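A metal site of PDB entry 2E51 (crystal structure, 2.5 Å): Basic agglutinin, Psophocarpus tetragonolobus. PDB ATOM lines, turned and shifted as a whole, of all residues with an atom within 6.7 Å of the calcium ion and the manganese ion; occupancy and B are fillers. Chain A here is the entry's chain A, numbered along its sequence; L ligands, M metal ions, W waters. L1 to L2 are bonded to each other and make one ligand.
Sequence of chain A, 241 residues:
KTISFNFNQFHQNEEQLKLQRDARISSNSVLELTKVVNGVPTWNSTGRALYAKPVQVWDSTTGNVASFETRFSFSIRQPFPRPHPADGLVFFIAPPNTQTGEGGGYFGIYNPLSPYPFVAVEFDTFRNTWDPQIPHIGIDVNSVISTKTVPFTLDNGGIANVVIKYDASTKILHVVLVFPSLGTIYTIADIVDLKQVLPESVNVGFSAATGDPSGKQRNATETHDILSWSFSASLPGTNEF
O2 of LG2 L2 lies within hydrogen-bond range of OD2 of Asp 87.
N of Gly 105 sits at hydrogen-bond distance from O2 of LG2 L2 (2.7 Å).
ND2 of Asn 128 sits at hydrogen-bond distance from O2 of LG2 L2 (3.3 Å).
The guanidinium group (NE) of Arg 127 sits at hydrogen-bond distance from the backbone carbonyl oxygen (O) of Asp 131, at 2.9 Å.
The backbone carbonyl oxygen of Gly 138 sits at hydrogen-bond distance from the backbone NH of Glu 122, 2.9 Å away.
OE1 of Glu 122 lies close to OD2 of Asp 140, at 2.5 Å.
Within 4 Å of the calcium ion: Asp 124, Phe 126, Asn 128 and Asp 131.
The nearest printed residue that does not touch the calcium ion is Gly 105 (4.4 Å).
Within 4 Å of the manganese ion: Glu 122, Asp 124, Asp 131 and His 136.
The nearest printed residue that does not touch the manganese ion is Val 144 (4.2 Å).
The calcium ion is bound by the side-chain carboxylate (OD2) of Asp 131, water W2, the backbone carbonyl oxygen (O) of Phe 126, the side-chain amide oxygen (OD1) of Asn 128, the side-chain carboxylate (OD2) of Asp 124 and the side-chain carboxylate (OD1) of Asp 124.
The calcium ion has six donor atoms within binding distance.
The manganese ion is bound by OD1 of Asp 131 (2.2 Å), OD2 of Asp 124 (2.3 Å), OE2 of Glu 122 (2.3 Å), water W1 (2.3 Å) and NE2 of His 136 (2.6 Å).
The manganese ion has five donor atoms within binding distance.
Water W2 lies within hydrogen-bond range of O of Gly 105 (2.7 Å) and NE1 of Trp 130 (3.3 Å).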
ATOM      1  N   ASP A  87      10.493   5.668  -2.858  1.00  0.00           N
ATOM      2  CA  ASP A  87      11.403   4.702  -3.452  1.00  0.00           C
ATOM      3  C   ASP A  87      12.836   4.945  -3.044  1.00  0.00           C
ATOM      4  O   ASP A  87      13.645   4.016  -2.966  1.00  0.00           O
ATOM      5  CB  ASP A  87      11.306   4.734  -4.971  1.00  0.00           C
ATOM      6  CG  ASP A  87      10.274   3.748  -5.496  1.00  0.00           C
ATOM      7  OD1 ASP A  87       9.139   4.178  -5.761  1.00  0.00           O
ATOM      8  OD2 ASP A  87      10.607   2.556  -5.615  1.00  0.00           O
ATOM      9  N   GLY A 104       9.294   6.062  -9.682  1.00  0.00           N
ATOM     10  CA  GLY A 104       9.457   4.780  -9.030  1.00  0.00           C
ATOM     11  C   GLY A 104      10.915   4.413  -8.767  1.00  0.00           C
ATOM     12  O   GLY A 104      11.727   5.275  -8.388  1.00  0.00           O
ATOM     13  N   GLY A 105      11.228   3.134  -8.980  1.00  0.00           N
ATOM     14  CA  GLY A 105      12.569   2.621  -8.759  1.00  0.00           C
ATOM     15  C   GLY A 105      13.603   3.211  -9.684  1.00  0.00           C
ATOM     16  O   GLY A 105      14.766   2.855  -9.589  1.00  0.00           O
ATOM     17  N   TYR A 106      13.183   4.098 -10.587  1.00  0.00           N
ATOM     18  CA  TYR A 106      14.117   4.759 -11.512  1.00  0.00           C
ATOM     19  C   TYR A 106      14.534   6.118 -10.966  1.00  0.00           C
ATOM     20  O   TYR A 106      15.318   6.843 -11.590  1.00  0.00           O
ATOM     21  CB  TYR A 106      13.472   4.892 -12.874  1.00  0.00           C
ATOM     22  CG  TYR A 106      13.324   3.566 -13.591  1.00  0.00           C
ATOM     23  CD1 TYR A 106      14.430   2.802 -13.920  1.00  0.00           C
ATOM     24  CD2 TYR A 106      12.055   3.068 -13.918  1.00  0.00           C
ATOM     25  CE1 TYR A 106      14.311   1.566 -14.563  1.00  0.00           C
ATOM     26  CE2 TYR A 106      11.909   1.823 -14.564  1.00  0.00           C
ATOM     27  CZ  TYR A 106      13.052   1.083 -14.888  1.00  0.00           C
ATOM     28  OH  TYR A 106      12.915  -0.128 -15.524  1.00  0.00           O
ATOM     29  N   PHE A 107      14.009   6.449  -9.784  1.00  0.00           N
ATOM     30  CA  PHE A 107      14.341   7.683  -9.077  1.00  0.00           C
ATOM     31  C   PHE A 107      14.196   8.989  -9.839  1.00  0.00           C
ATOM     32  O   PHE A 107      14.510  10.047  -9.312  1.00  0.00           O
ATOM     33  CB  PHE A 107      15.783   7.591  -8.548  1.00  0.00           C
ATOM     34  CG  PHE A 107      16.100   6.295  -7.824  1.00  0.00           C
ATOM     35  CD1 PHE A 107      15.532   6.014  -6.613  1.00  0.00           C
ATOM     36  CD2 PHE A 107      17.023   5.404  -8.353  1.00  0.00           C
ATOM     37  CE1 PHE A 107      15.881   4.848  -5.903  1.00  0.00           C
ATOM     38  CE2 PHE A 107      17.370   4.272  -7.676  1.00  0.00           C
ATOM     39  CZ  PHE A 107      16.804   3.978  -6.438  1.00  0.00           C
ATOM     40  N   GLU A 122      22.838   6.070  -4.844  1.00  0.00           N
ATOM     41  CA  GLU A 122      21.472   5.934  -4.391  1.00  0.00           C
ATOM     42  C   GLU A 122      21.308   5.483  -2.934  1.00  0.00           C
ATOM     43  O   GLU A 122      22.158   4.794  -2.369  1.00  0.00           O
ATOM     44  CB  GLU A 122      20.743   4.931  -5.261  1.00  0.00           C
ATOM     45  CG  GLU A 122      21.295   3.533  -5.106  1.00  0.00           C
ATOM     46  CD  GLU A 122      20.506   2.481  -5.877  1.00  0.00           C
ATOM     47  OE1 GLU A 122      20.229   2.704  -7.085  1.00  0.00           O
ATOM     48  OE2 GLU A 122      20.194   1.446  -5.263  1.00  0.00           O
ATOM     49  N   ASP A 124      18.444   3.660  -1.641  1.00  0.00           N
ATOM     50  CA  ASP A 124      17.292   2.924  -2.074  1.00  0.00           C
ATOM     51  C   ASP A 124      16.479   2.337  -0.949  1.00  0.00           C
ATOM     52  O   ASP A 124      17.005   1.579  -0.134  1.00  0.00           O
ATOM     53  CB  ASP A 124      17.770   1.826  -3.007  1.00  0.00           C
ATOM     54  CG  ASP A 124      16.676   1.254  -3.849  1.00  0.00           C
ATOM     55  OD1 ASP A 124      15.492   1.524  -3.569  1.00  0.00           O
ATOM     56  OD2 ASP A 124      17.011   0.519  -4.788  1.00  0.00           O
ATOM     57  N   THR A 125      15.181   2.636  -0.923  1.00  0.00           N
ATOM     58  CA  THR A 125      14.341   2.138   0.151  1.00  0.00           C
ATOM     59  C   THR A 125      13.295   1.098  -0.259  1.00  0.00           C
ATOM     60  O   THR A 125      12.600   0.549   0.593  1.00  0.00           O
ATOM     61  CB  THR A 125      13.637   3.290   0.825  1.00  0.00           C
ATOM     62  OG1 THR A 125      12.922   4.035  -0.173  1.00  0.00           O
ATOM     63  CG2 THR A 125      14.642   4.202   1.506  1.00  0.00           C
ATOM     64  N   PHE A 126      13.163   0.825  -1.551  1.00  0.00           N
ATOM     65  CA  PHE A 126      12.194  -0.140  -2.027  1.00  0.00           C
ATOM     66  C   PHE A 126      12.886  -1.189  -2.871  1.00  0.00           C
ATOM     67  O   PHE A 126      13.666  -0.861  -3.793  1.00  0.00           O
ATOM     68  CB  PHE A 126      11.114   0.527  -2.858  1.00  0.00           C
ATOM     69  CG  PHE A 126      10.166  -0.453  -3.491  1.00  0.00           C
ATOM     70  CD1 PHE A 126       9.063  -0.915  -2.787  1.00  0.00           C
ATOM     71  CD2 PHE A 126      10.394  -0.916  -4.783  1.00  0.00           C
ATOM     72  CE1 PHE A 126       8.187  -1.841  -3.361  1.00  0.00           C
ATOM     73  CE2 PHE A 126       9.533  -1.836  -5.370  1.00  0.00           C
ATOM     74  CZ  PHE A 126       8.430  -2.298  -4.665  1.00  0.00           C
ATOM     75  N   ARG A 127      12.591  -2.442  -2.574  1.00  0.00           N
ATOM     76  CA  ARG A 127      13.226  -3.529  -3.311  1.00  0.00           C
ATOM     77  C   ARG A 127      12.571  -3.913  -4.626  1.00  0.00           C
ATOM     78  O   ARG A 127      11.571  -4.581  -4.623  1.00  0.00           O
ATOM     79  CB  ARG A 127      13.352  -4.776  -2.417  1.00  0.00           C
ATOM     80  CG  ARG A 127      14.088  -5.883  -3.113  1.00  0.00           C
ATOM     81  CD  ARG A 127      14.498  -7.011  -2.161  1.00  0.00           C
ATOM     82  NE  ARG A 127      15.328  -7.998  -2.869  1.00  0.00           N
ATOM     83  CZ  ARG A 127      16.001  -8.967  -2.256  1.00  0.00           C
ATOM     84  NH1 ARG A 127      15.961  -9.087  -0.946  1.00  0.00           N
ATOM     85  NH2 ARG A 127      16.722  -9.812  -2.973  1.00  0.00           N
ATOM     86  N   ASN A 128      13.159  -3.482  -5.730  1.00  0.00           N
ATOM     87  CA  ASN A 128      12.644  -3.837  -7.048  1.00  0.00           C
ATOM     88  C   ASN A 128      13.185  -5.205  -7.424  1.00  0.00           C
ATOM     89  O   ASN A 128      13.981  -5.786  -6.697  1.00  0.00           O
ATOM     90  CB  ASN A 128      13.052  -2.825  -8.098  1.00  0.00           C
ATOM     91  CG  ASN A 128      12.418  -1.470  -7.878  1.00  0.00           C
ATOM     92  OD1 ASN A 128      12.791  -0.737  -6.935  1.00  0.00           O
ATOM     93  ND2 ASN A 128      11.442  -1.116  -8.722  1.00  0.00           N
ATOM     94  N   TRP A 130      15.356  -6.027  -9.509  1.00  0.00           N
ATOM     95  CA  TRP A 130      16.810  -5.963  -9.677  1.00  0.00           C
ATOM     96  C   TRP A 130      17.609  -5.609  -8.419  1.00  0.00           C
ATOM     97  O   TRP A 130      18.835  -5.549  -8.468  1.00  0.00           O
ATOM     98  CB  TRP A 130      17.124  -4.950 -10.769  1.00  0.00           C
ATOM     99  CG  TRP A 130      16.633  -3.562 -10.437  1.00  0.00           C
ATOM    100  CD1 TRP A 130      17.168  -2.685  -9.513  1.00  0.00           C
ATOM    101  CD2 TRP A 130      15.484  -2.906 -10.975  1.00  0.00           C
ATOM    102  NE1 TRP A 130      16.407  -1.547  -9.442  1.00  0.00           N
ATOM    103  CE2 TRP A 130      15.369  -1.648 -10.331  1.00  0.00           C
ATOM    104  CE3 TRP A 130      14.525  -3.252 -11.937  1.00  0.00           C
ATOM    105  CZ2 TRP A 130      14.344  -0.752 -10.618  1.00  0.00           C
ATOM    106  CZ3 TRP A 130      13.493  -2.357 -12.232  1.00  0.00           C
ATOM    107  CH2 TRP A 130      13.418  -1.128 -11.574  1.00  0.00           C
ATOM    108  N   ASP A 131      16.898  -5.393  -7.309  1.00  0.00           N
ATOM    109  CA  ASP A 131      17.510  -5.000  -6.039  1.00  0.00           C
ATOM    110  C   ASP A 131      17.811  -6.054  -5.016  1.00  0.00           C
ATOM    111  O   ASP A 131      17.137  -7.088  -4.946  1.00  0.00           O
ATOM    112  CB  ASP A 131      16.597  -4.016  -5.251  1.00  0.00           C
ATOM    113  CG  ASP A 131      16.713  -2.572  -5.706  1.00  0.00           C
ATOM    114  OD1 ASP A 131      17.802  -2.184  -6.162  1.00  0.00           O
ATOM    115  OD2 ASP A 131      15.698  -1.850  -5.546  1.00  0.00           O
ATOM    116  N   PRO A 132      18.835  -5.795  -4.179  1.00  0.00           N
ATOM    117  CA  PRO A 132      19.230  -6.702  -3.094  1.00  0.00           C
ATOM    118  C   PRO A 132      18.386  -6.164  -1.936  1.00  0.00           C
ATOM    119  O   PRO A 132      17.624  -5.234  -2.118  1.00  0.00           O
ATOM    120  CB  PRO A 132      20.722  -6.413  -2.913  1.00  0.00           C
ATOM    121  CG  PRO A 132      20.848  -4.990  -3.320  1.00  0.00           C
ATOM    122  CD  PRO A 132      19.965  -4.938  -4.576  1.00  0.00           C
ATOM    123  N   ILE A 134      16.766  -4.116   1.033  1.00  0.00           N
ATOM    124  CA  ILE A 134      16.762  -2.676   1.288  1.00  0.00           C
ATOM    125  C   ILE A 134      16.610  -2.402   2.782  1.00  0.00           C
ATOM    126  O   ILE A 134      16.126  -3.240   3.515  1.00  0.00           O
ATOM    127  CB  ILE A 134      15.606  -1.932   0.488  1.00  0.00           C
ATOM    128  CG1 ILE A 134      14.236  -2.556   0.740  1.00  0.00           C
ATOM    129  CG2 ILE A 134      15.897  -1.967  -0.976  1.00  0.00           C
ATOM    130  CD1 ILE A 134      13.644  -2.318   2.166  1.00  0.00           C
ATOM    131  N   HIS A 136      19.544   0.127   1.001  1.00  0.00           N
ATOM    132  CA  HIS A 136      20.936  -0.054   0.651  1.00  0.00           C
ATOM    133  C   HIS A 136      21.511   1.176  -0.035  1.00  0.00           C
ATOM    134  O   HIS A 136      20.795   1.999  -0.607  1.00  0.00           O
ATOM    135  CB  HIS A 136      21.141  -1.305  -0.250  1.00  0.00           C
ATOM    136  CG  HIS A 136      20.347  -1.327  -1.521  1.00  0.00           C
ATOM    137  ND1 HIS A 136      19.235  -2.119  -1.700  1.00  0.00           N
ATOM    138  CD2 HIS A 136      20.522  -0.667  -2.696  1.00  0.00           C
ATOM    139  CE1 HIS A 136      18.764  -1.964  -2.920  1.00  0.00           C
ATOM    140  NE2 HIS A 136      19.519  -1.088  -3.554  1.00  0.00           N
ATOM    141  N   GLY A 138      23.951   2.388  -2.961  1.00  0.00           N
ATOM    142  CA  GLY A 138      24.370   1.778  -4.203  1.00  0.00           C
ATOM    143  C   GLY A 138      25.072   2.769  -5.108  1.00  0.00           C
ATOM    144  O   GLY A 138      24.771   3.957  -5.066  1.00  0.00           O
ATOM    145  N   ASP A 140      25.602   3.661  -8.900  1.00  0.00           N
ATOM    146  CA  ASP A 140      25.013   3.407 -10.206  1.00  0.00           C
ATOM    147  C   ASP A 140      25.733   4.110 -11.334  1.00  0.00           C
ATOM    148  O   ASP A 140      26.081   5.271 -11.223  1.00  0.00           O
ATOM    149  CB  ASP A 140      23.525   3.832 -10.224  1.00  0.00           C
ATOM    150  CG  ASP A 140      22.686   3.103  -9.178  1.00  0.00           C
ATOM    151  OD1 ASP A 140      23.235   2.342  -8.355  1.00  0.00           O
ATOM    152  OD2 ASP A 140      21.458   3.281  -9.193  1.00  0.00           O
ATOM    153  N   VAL A 144      20.240   1.738 -12.989  1.00  0.00           N
ATOM    154  CA  VAL A 144      19.906   1.655 -11.581  1.00  0.00           C
ATOM    155  C   VAL A 144      20.259   0.287 -11.024  1.00  0.00           C
ATOM    156  O   VAL A 144      19.943  -0.027  -9.892  1.00  0.00           O
ATOM    157  CB  VAL A 144      18.415   1.957 -11.347  1.00  0.00           C
ATOM    158  CG1 VAL A 144      18.215   3.474 -11.227  1.00  0.00           C
ATOM    159  CG2 VAL A 144      17.600   1.411 -12.524  1.00  0.00           C
ATOM    160  N   ILE A 145      20.893  -0.539 -11.845  1.00  0.00           N
ATOM    161  CA  ILE A 145      21.335  -1.858 -11.384  1.00  0.00           C
ATOM    162  C   ILE A 145      22.771  -1.619 -10.912  1.00  0.00           C
ATOM    163  O   ILE A 145      23.717  -1.677 -11.687  1.00  0.00           O
ATOM    164  CB  ILE A 145      21.329  -2.871 -12.534  1.00  0.00           C
ATOM    165  CG1 ILE A 145      19.916  -3.002 -13.087  1.00  0.00           C
ATOM    166  CG2 ILE A 145      21.797  -4.224 -12.060  1.00  0.00           C
ATOM    167  CD1 ILE A 145      19.841  -3.965 -14.244  1.00  0.00           C
ATOM    168  N   SER A 146      22.903  -1.304  -9.617  1.00  0.00           N
ATOM    169  CA  SER A 146      24.157  -0.938  -8.975  1.00  0.00           C
ATOM    170  C   SER A 146      25.338  -1.829  -9.231  1.00  0.00           C
ATOM    171  O   SER A 146      25.213  -3.042  -9.276  1.00  0.00           O
ATOM    172  CB  SER A 146      23.947  -0.824  -7.463  1.00  0.00           C
ATOM    173  OG  SER A 146      22.833   0.014  -7.171  1.00  0.00           O
ATOM    174  N   THR A 149      26.812  -2.486  -3.899  1.00  0.00           N
ATOM    175  CA  THR A 149      25.736  -2.186  -2.969  1.00  0.00           C
ATOM    176  C   THR A 149      26.151  -2.483  -1.517  1.00  0.00           C
ATOM    177  O   THR A 149      27.017  -3.328  -1.256  1.00  0.00           O
ATOM    178  CB  THR A 149      24.495  -3.063  -3.363  1.00  0.00           C
ATOM    179  OG1 THR A 149      23.651  -2.338  -4.280  1.00  0.00           O
ATOM    180  CG2 THR A 149      23.702  -3.479  -2.151  1.00  0.00           C
HETATM  181  C1  LIG L   1       3.890  -3.828  -9.960  1.00  0.00           C
HETATM  182  C2  LIG L   1       4.619  -2.544  -9.478  1.00  0.00           C
HETATM  183  C3  LIG L   1       6.060  -2.878  -9.000  1.00  0.00           C
HETATM  184  C4  LIG L   1       5.999  -3.979  -7.948  1.00  0.00           C
HETATM  185  C5  LIG L   1       5.262  -5.219  -8.498  1.00  0.00           C
HETATM  186  C6  LIG L   1       5.136  -6.311  -7.436  1.00  0.00           C
HETATM  187  O1  LIG L   1       4.493  -4.325 -11.102  1.00  0.00           O
HETATM  188  O2  LIG L   1       4.669  -1.586 -10.528  1.00  0.00           O
HETATM  189  O3  LIG L   1       6.776  -1.732  -8.438  1.00  0.00           O
HETATM  190  O4  LIG L   1       5.341  -3.480  -6.788  1.00  0.00           O
HETATM  191  O5  LIG L   1       3.912  -4.854  -8.939  1.00  0.00           O
HETATM  192  O6  LIG L   1       4.483  -7.461  -7.929  1.00  0.00           O
HETATM  193  O1  LG2 L   2       5.596   0.115  -7.486  1.00  0.00           O
HETATM  194  C1  LG2 L   2       6.349  -0.383  -8.618  1.00  0.00           C
HETATM  195  C2  LG2 L   2       7.590   0.526  -8.882  1.00  0.00           C
HETATM  196  N1  LG2 L   2       8.388   0.000  -9.993  1.00  0.00           N
HETATM  197  C3  LG2 L   2       8.429   0.603  -7.568  1.00  0.00           C
HETATM  198  O2  LG2 L   2       9.594   1.383  -7.742  1.00  0.00           O
HETATM  199  C4  LG2 L   2       7.555   1.141  -6.412  1.00  0.00           C
HETATM  200  O3  LG2 L   2       7.126   2.473  -6.678  1.00  0.00           O
HETATM  201  C5  LG2 L   2       6.322   0.230  -6.232  1.00  0.00           C
HETATM  202  C6  LG2 L   2       5.364   0.776  -5.166  1.00  0.00           C
HETATM  203  O4  LG2 L   2       4.237  -0.057  -4.959  1.00  0.00           O
HETATM  204  C7  LG2 L   2       8.816   0.772 -11.006  1.00  0.00           C
HETATM  205  O5  LG2 L   2       8.619   1.994 -11.082  1.00  0.00           O
HETATM  206  C8  LG2 L   2       9.613   0.075 -12.103  1.00  0.00           C
HETATM  207 CA    CA M   1      14.611   0.249  -5.689  1.00  0.00          CA
HETATM  208 MN    MN M   2      18.832  -0.269  -5.882  1.00  0.00          MN
HETATM  209  O   HOH W   1      20.729  -1.435  -6.457  1.00  0.00           O
HETATM  210  O   HOH W   2      15.619   1.101  -7.681  1.00  0.00           O
